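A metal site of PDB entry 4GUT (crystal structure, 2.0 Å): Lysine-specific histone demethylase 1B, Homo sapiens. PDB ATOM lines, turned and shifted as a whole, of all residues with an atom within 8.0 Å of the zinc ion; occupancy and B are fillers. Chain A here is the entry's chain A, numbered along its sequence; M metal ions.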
ATOM      1  N   VAL A  18     -12.692 -26.250  34.861  1.00  0.00           N
ATOM      2  CA  VAL A  18     -12.197 -27.262  33.916  1.00  0.00           C
ATOM      3  C   VAL A  18     -12.185 -26.649  32.519  1.00  0.00           C
ATOM      4  O   VAL A  18     -12.984 -25.756  32.237  1.00  0.00           O
ATOM      5  CB  VAL A  18     -13.031 -28.564  33.959  1.00  0.00           C
ATOM      6  CG1 VAL A  18     -13.143 -29.083  35.387  1.00  0.00           C
ATOM      7  CG2 VAL A  18     -14.409 -28.356  33.352  1.00  0.00           C
ATOM      8  N   CYS A  19     -11.284 -27.100  31.660  1.00  0.00           N
ATOM      9  CA  CYS A  19     -11.203 -26.540  30.312  1.00  0.00           C
ATOM     10  C   CYS A  19     -12.169 -27.208  29.334  1.00  0.00           C
ATOM     11  O   CYS A  19     -12.232 -28.434  29.259  1.00  0.00           O
ATOM     12  CB  CYS A  19      -9.788 -26.623  29.774  1.00  0.00           C
ATOM     13  SG  CYS A  19      -9.611 -25.917  28.127  1.00  0.00           S
ATOM     14  N   PHE A  20     -12.919 -26.402  28.579  1.00  0.00           N
ATOM     15  CA  PHE A  20     -13.916 -26.944  27.667  1.00  0.00           C
ATOM     16  C   PHE A  20     -13.354 -27.139  26.262  1.00  0.00           C
ATOM     17  O   PHE A  20     -13.954 -27.843  25.445  1.00  0.00           O
ATOM     18  CB  PHE A  20     -15.157 -26.034  27.605  1.00  0.00           C
ATOM     19  CG  PHE A  20     -14.889 -24.673  27.012  1.00  0.00           C
ATOM     20  CD1 PHE A  20     -14.872 -23.544  27.813  1.00  0.00           C
ATOM     21  CD2 PHE A  20     -14.648 -24.534  25.639  1.00  0.00           C
ATOM     22  CE1 PHE A  20     -14.618 -22.297  27.276  1.00  0.00           C
ATOM     23  CE2 PHE A  20     -14.394 -23.287  25.102  1.00  0.00           C
ATOM     24  CZ  PHE A  20     -14.368 -22.171  25.919  1.00  0.00           C
ATOM     25  N   ALA A  21     -12.221 -26.511  25.969  1.00  0.00           N
ATOM     26  CA  ALA A  21     -11.683 -26.537  24.616  1.00  0.00           C
ATOM     27  C   ALA A  21     -10.963 -27.839  24.304  1.00  0.00           C
ATOM     28  O   ALA A  21     -11.195 -28.435  23.245  1.00  0.00           O
ATOM     29  CB  ALA A  21     -10.775 -25.346  24.372  1.00  0.00           C
ATOM     30  N   SER A  22     -10.103 -28.281  25.235  1.00  0.00           N
ATOM     31  CA  SER A  22      -9.182 -29.415  25.038  1.00  0.00           C
ATOM     32  C   SER A  22      -8.748 -29.502  23.579  1.00  0.00           C
ATOM     33  O   SER A  22      -8.878 -30.535  22.923  1.00  0.00           O
ATOM     34  CB  SER A  22      -9.780 -30.733  25.548  1.00  0.00           C
ATOM     35  OG  SER A  22     -10.835 -31.187  24.718  1.00  0.00           O
ATOM     36  N   ALA A  23      -8.260 -28.371  23.093  1.00  0.00           N
ATOM     37  CA  ALA A  23      -7.845 -28.222  21.709  1.00  0.00           C
ATOM     38  C   ALA A  23      -6.344 -28.450  21.605  1.00  0.00           C
ATOM     39  O   ALA A  23      -5.862 -28.916  20.575  1.00  0.00           O
ATOM     40  CB  ALA A  23      -8.198 -26.830  21.232  1.00  0.00           C
ATOM     41  N   SER A  24      -5.612 -28.099  22.657  1.00  0.00           N
ATOM     42  CA  SER A  24      -4.163 -28.294  22.695  1.00  0.00           C
ATOM     43  C   SER A  24      -3.817 -29.632  23.336  1.00  0.00           C
ATOM     44  O   SER A  24      -4.424 -30.027  24.334  1.00  0.00           O
ATOM     45  CB  SER A  24      -3.494 -27.139  23.449  1.00  0.00           C
ATOM     46  OG  SER A  24      -2.171 -27.470  23.838  1.00  0.00           O
ATOM     47  N   GLU A  25      -2.839 -30.328  22.758  1.00  0.00           N
ATOM     48  CA  GLU A  25      -2.255 -31.518  23.384  1.00  0.00           C
ATOM     49  C   GLU A  25      -1.756 -31.209  24.789  1.00  0.00           C
ATOM     50  O   GLU A  25      -1.597 -32.125  25.608  1.00  0.00           O
ATOM     51  CB  GLU A  25      -1.126 -32.117  22.517  1.00  0.00           C
ATOM     52  CG  GLU A  25       0.043 -31.183  22.229  1.00  0.00           C
ATOM     53  CD  GLU A  25      -0.328 -30.030  21.312  1.00  0.00           C
ATOM     54  OE1 GLU A  25      -0.546 -30.271  20.109  1.00  0.00           O
ATOM     55  OE2 GLU A  25      -0.412 -28.882  21.806  1.00  0.00           O
ATOM     56  N   ARG A  26      -1.535 -29.926  25.080  1.00  0.00           N
ATOM     57  CA  ARG A  26      -1.015 -29.475  26.372  1.00  0.00           C
ATOM     58  C   ARG A  26      -2.100 -28.966  27.349  1.00  0.00           C
ATOM     59  O   ARG A  26      -1.795 -28.467  28.429  1.00  0.00           O
ATOM     60  CB  ARG A  26       0.107 -28.452  26.154  1.00  0.00           C
ATOM     61  CG  ARG A  26       1.106 -28.876  25.075  1.00  0.00           C
ATOM     62  CD  ARG A  26       2.399 -28.067  25.049  1.00  0.00           C
ATOM     63  NE  ARG A  26       3.096 -28.120  26.334  1.00  0.00           N
ATOM     64  CZ  ARG A  26       4.416 -28.014  26.504  1.00  0.00           C
ATOM     65  NH1 ARG A  26       5.230 -27.849  25.459  1.00  0.00           N
ATOM     66  NH2 ARG A  26       4.912 -28.076  27.717  1.00  0.00           N
ATOM     67  N   CYS A  27      -3.373 -29.122  26.965  1.00  0.00           N
ATOM     68  CA  CYS A  27      -4.509 -28.684  27.774  1.00  0.00           C
ATOM     69  C   CYS A  27      -4.377 -29.038  29.246  1.00  0.00           C
ATOM     70  O   CYS A  27      -4.049 -30.181  29.602  1.00  0.00           O
ATOM     71  CB  CYS A  27      -5.821 -29.265  27.214  1.00  0.00           C
ATOM     72  SG  CYS A  27      -7.308 -28.871  28.175  1.00  0.00           S
ATOM     73  N   ALA A  28      -4.647 -28.062  30.110  1.00  0.00           N
ATOM     74  CA  ALA A  28      -4.541 -28.271  31.554  1.00  0.00           C
ATOM     75  C   ALA A  28      -5.681 -29.113  32.113  1.00  0.00           C
ATOM     76  O   ALA A  28      -5.635 -29.533  33.268  1.00  0.00           O
ATOM     77  CB  ALA A  28      -4.480 -26.925  32.275  1.00  0.00           C
ATOM     78  N   LYS A  29      -6.705 -29.363  31.287  1.00  0.00           N
ATOM     79  CA  LYS A  29      -7.858 -30.170  31.670  1.00  0.00           C
ATOM     80  C   LYS A  29      -8.548 -29.597  32.906  1.00  0.00           C
ATOM     81  O   LYS A  29      -9.111 -28.506  32.866  1.00  0.00           O
ATOM     82  CB  LYS A  29      -7.460 -31.642  31.905  1.00  0.00           C
ATOM     83  CG  LYS A  29      -6.579 -32.253  30.834  1.00  0.00           C
ATOM     84  CD  LYS A  29      -7.399 -33.003  29.797  1.00  0.00           C
ATOM     85  CE  LYS A  29      -6.498 -33.820  28.890  1.00  0.00           C
ATOM     86  NZ  LYS A  29      -5.643 -34.760  29.686  1.00  0.00           N
ATOM     87  N   ASN A  30      -8.488 -30.338  34.015  1.00  0.00           N
ATOM     88  CA  ASN A  30      -9.024 -29.886  35.293  1.00  0.00           C
ATOM     89  C   ASN A  30      -7.923 -29.541  36.298  1.00  0.00           C
ATOM     90  O   ASN A  30      -8.191 -29.319  37.477  1.00  0.00           O
ATOM     91  CB  ASN A  30      -9.993 -30.932  35.870  1.00  0.00           C
ATOM     92  CG  ASN A  30      -9.316 -32.262  36.212  1.00  0.00           C
ATOM     93  OD1 ASN A  30      -9.900 -33.078  36.916  1.00  0.00           O
ATOM     94  ND2 ASN A  30      -8.112 -32.481  35.702  1.00  0.00           N
ATOM     95  N   THR A  33      -3.132 -24.471  35.748  1.00  0.00           N
ATOM     96  CA  THR A  33      -2.661 -23.758  34.564  1.00  0.00           C
ATOM     97  C   THR A  33      -2.271 -22.340  34.950  1.00  0.00           C
ATOM     98  O   THR A  33      -2.720 -21.826  35.985  1.00  0.00           O
ATOM     99  CB  THR A  33      -3.716 -23.693  33.428  1.00  0.00           C
ATOM    100  OG1 THR A  33      -3.193 -22.934  32.319  1.00  0.00           O
ATOM    101  CG2 THR A  33      -5.017 -23.046  33.904  1.00  0.00           C
ATOM    102  N   TRP A  36      -6.812 -19.250  34.051  1.00  0.00           N
ATOM    103  CA  TRP A  36      -8.132 -19.747  33.697  1.00  0.00           C
ATOM    104  C   TRP A  36      -8.965 -18.654  33.105  1.00  0.00           C
ATOM    105  O   TRP A  36      -9.284 -17.670  33.780  1.00  0.00           O
ATOM    106  CB  TRP A  36      -8.821 -20.347  34.912  1.00  0.00           C
ATOM    107  CG  TRP A  36      -8.426 -21.775  35.189  1.00  0.00           C
ATOM    108  CD1 TRP A  36      -7.798 -22.286  36.321  1.00  0.00           C
ATOM    109  CD2 TRP A  36      -8.606 -22.930  34.287  1.00  0.00           C
ATOM    110  NE1 TRP A  36      -7.586 -23.639  36.190  1.00  0.00           N
ATOM    111  CE2 TRP A  36      -8.043 -24.085  35.002  1.00  0.00           C
ATOM    112  CE3 TRP A  36      -9.151 -23.112  33.030  1.00  0.00           C
ATOM    113  CZ2 TRP A  36      -8.053 -25.362  34.448  1.00  0.00           C
ATOM    114  CZ3 TRP A  36      -9.149 -24.402  32.479  1.00  0.00           C
ATOM    115  CH2 TRP A  36      -8.611 -25.497  33.168  1.00  0.00           C
ATOM    116  N   HIS A  44     -14.855 -22.148  31.322  1.00  0.00           N
ATOM    117  CA  HIS A  44     -13.501 -21.596  31.229  1.00  0.00           C
ATOM    118  C   HIS A  44     -12.651 -22.421  30.326  1.00  0.00           C
ATOM    119  O   HIS A  44     -12.901 -23.606  30.116  1.00  0.00           O
ATOM    120  CB  HIS A  44     -12.855 -21.553  32.605  1.00  0.00           C
ATOM    121  CG  HIS A  44     -13.698 -20.908  33.668  1.00  0.00           C
ATOM    122  ND1 HIS A  44     -14.667 -21.566  34.329  1.00  0.00           N
ATOM    123  CD2 HIS A  44     -13.692 -19.612  34.171  1.00  0.00           C
ATOM    124  CE1 HIS A  44     -15.248 -20.733  35.208  1.00  0.00           C
ATOM    125  NE2 HIS A  44     -14.655 -19.538  35.108  1.00  0.00           N
ATOM    126  N   PHE A  45     -11.606 -21.792  29.781  1.00  0.00           N
ATOM    127  CA  PHE A  45     -10.592 -22.538  29.045  1.00  0.00           C
ATOM    128  C   PHE A  45      -9.182 -22.174  29.524  1.00  0.00           C
ATOM    129  O   PHE A  45      -8.930 -21.039  29.936  1.00  0.00           O
ATOM    130  CB  PHE A  45     -10.737 -22.380  27.521  1.00  0.00           C
ATOM    131  CG  PHE A  45     -10.616 -20.972  27.023  1.00  0.00           C
ATOM    132  CD1 PHE A  45      -9.504 -20.568  26.290  1.00  0.00           C
ATOM    133  CD2 PHE A  45     -11.646 -20.037  27.245  1.00  0.00           C
ATOM    134  CE1 PHE A  45      -9.400 -19.276  25.804  1.00  0.00           C
ATOM    135  CE2 PHE A  45     -11.544 -18.738  26.766  1.00  0.00           C
ATOM    136  CZ  PHE A  45     -10.420 -18.354  26.042  1.00  0.00           C
ATOM    137  N   CYS A  46      -8.286 -23.151  29.451  1.00  0.00           N
ATOM    138  CA  CYS A  46      -6.935 -23.029  30.000  1.00  0.00           C
ATOM    139  C   CYS A  46      -6.013 -22.229  29.085  1.00  0.00           C
ATOM    140  O   CYS A  46      -6.280 -22.063  27.885  1.00  0.00           O
ATOM    141  CB  CYS A  46      -6.325 -24.414  30.244  1.00  0.00           C
ATOM    142  SG  CYS A  46      -5.796 -25.211  28.715  1.00  0.00           S
ATOM    143  N   ASN A  47      -4.913 -21.756  29.658  1.00  0.00           N
ATOM    144  CA  ASN A  47      -3.942 -20.914  28.953  1.00  0.00           C
ATOM    145  C   ASN A  47      -3.335 -21.499  27.674  1.00  0.00           C
ATOM    146  O   ASN A  47      -3.092 -20.775  26.714  1.00  0.00           O
ATOM    147  CB  ASN A  47      -2.825 -20.476  29.910  1.00  0.00           C
ATOM    148  CG  ASN A  47      -1.992 -19.355  29.343  1.00  0.00           C
ATOM    149  OD1 ASN A  47      -0.823 -19.545  28.999  1.00  0.00           O
ATOM    150  ND2 ASN A  47      -2.596 -18.165  29.217  1.00  0.00           N
ATOM    151  N   GLU A  48      -3.053 -22.802  27.677  1.00  0.00           N
ATOM    152  CA  GLU A  48      -2.427 -23.446  26.510  1.00  0.00           C
ATOM    153  C   GLU A  48      -3.398 -23.656  25.362  1.00  0.00           C
ATOM    154  O   GLU A  48      -3.005 -23.617  24.190  1.00  0.00           O
ATOM    155  CB  GLU A  48      -1.748 -24.767  26.888  1.00  0.00           C
ATOM    156  CG  GLU A  48      -2.304 -25.455  28.121  1.00  0.00           C
ATOM    157  CD  GLU A  48      -1.728 -24.910  29.424  1.00  0.00           C
ATOM    158  OE1 GLU A  48      -2.522 -24.534  30.325  1.00  0.00           O
ATOM    159  OE2 GLU A  48      -0.494 -24.854  29.542  1.00  0.00           O
ATOM    160  N   CYS A  49      -4.676 -23.889  25.683  1.00  0.00           N
ATOM    161  CA  CYS A  49      -5.706 -23.917  24.653  1.00  0.00           C
ATOM    162  C   CYS A  49      -5.899 -22.483  24.111  1.00  0.00           C
ATOM    163  O   CYS A  49      -6.066 -22.289  22.900  1.00  0.00           O
ATOM    164  CB  CYS A  49      -7.011 -24.512  25.194  1.00  0.00           C
ATOM    165  SG  CYS A  49      -6.911 -26.260  25.706  1.00  0.00           S
ATOM    166  N   PHE A  50      -5.849 -21.496  25.012  1.00  0.00           N
ATOM    167  CA  PHE A  50      -5.823 -20.076  24.633  1.00  0.00           C
ATOM    168  C   PHE A  50      -4.727 -19.878  23.589  1.00  0.00           C
ATOM    169  O   PHE A  50      -5.009 -19.483  22.456  1.00  0.00           O
ATOM    170  CB  PHE A  50      -5.592 -19.196  25.870  1.00  0.00           C
ATOM    171  CG  PHE A  50      -5.532 -17.711  25.583  1.00  0.00           C
ATOM    172  CD1 PHE A  50      -6.688 -16.938  25.560  1.00  0.00           C
ATOM    173  CD2 PHE A  50      -4.303 -17.074  25.373  1.00  0.00           C
ATOM    174  CE1 PHE A  50      -6.636 -15.575  25.308  1.00  0.00           C
ATOM    175  CE2 PHE A  50      -4.241 -15.709  25.123  1.00  0.00           C
ATOM    176  CZ  PHE A  50      -5.413 -14.953  25.083  1.00  0.00           C
ATOM    177  N   HIS A  52      -3.040 -22.154  21.916  1.00  0.00           N
ATOM    178  CA  HIS A  52      -3.159 -23.058  20.758  1.00  0.00           C
ATOM    179  C   HIS A  52      -3.766 -22.383  19.549  1.00  0.00           C
ATOM    180  O   HIS A  52      -3.411 -22.685  18.408  1.00  0.00           O
ATOM    181  CB  HIS A  52      -3.955 -24.316  21.124  1.00  0.00           C
ATOM    182  CG  HIS A  52      -4.055 -25.331  20.012  1.00  0.00           C
ATOM    183  ND1 HIS A  52      -5.170 -25.490  19.269  1.00  0.00           N
ATOM    184  CD2 HIS A  52      -3.122 -26.244  19.514  1.00  0.00           C
ATOM    185  CE1 HIS A  52      -4.963 -26.463  18.351  1.00  0.00           C
ATOM    186  NE2 HIS A  52      -3.712 -26.918  18.505  1.00  0.00           N
HETATM  187 ZN    ZN M   1      -7.435 -26.528  27.610  1.00  0.00          ZN
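SG of Cys 27 lies close to N of Lys 29 (3.2 Å).
SG of Cys 49 lies close to N of Ala 23 (3.6 Å).
The side-chain sulfur (SG) of Cys 19 lies close to the backbone NH (N) of Ala 21 (3.4 Å).
The side-chain sulfur (SG) of Cys 46 sits close to the backbone NH (N) of Ala 28 (3.4 Å).
The side-chain sulfur of Cys 46 lies close to the side-chain carboxylate of Glu 48, 3.7 Å away.
The side-chain sulfur (SG) of Cys 19 lies close to the backbone NH (N) of Ser 22 (3.8 Å).
The side-chain sulfur (SG) of Cys 49 sits close to the backbone NH (N) of Ser 24.
The backbone carbonyl oxygen (O) of Lys 29 is in hydrogen-bond range of the backbone NH (N) of Cys 19, 2.9 Å away.
The zinc ion is bound by the side-chain sulfur of Cys 49 (2.0 Å), the side-chain sulfur of Cys 19 (2.3 Å), the side-chain sulfur of Cys 46 (2.4 Å) and the side-chain sulfur of Cys 27 (2.4 Å).
The zinc ion has four donor atoms within binding distance.
Ser 22 touches the zinc ion (N to ZN, 3.98 Å).
Of the 23 residues printed, 5 come within 4 Å of the zinc ion.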
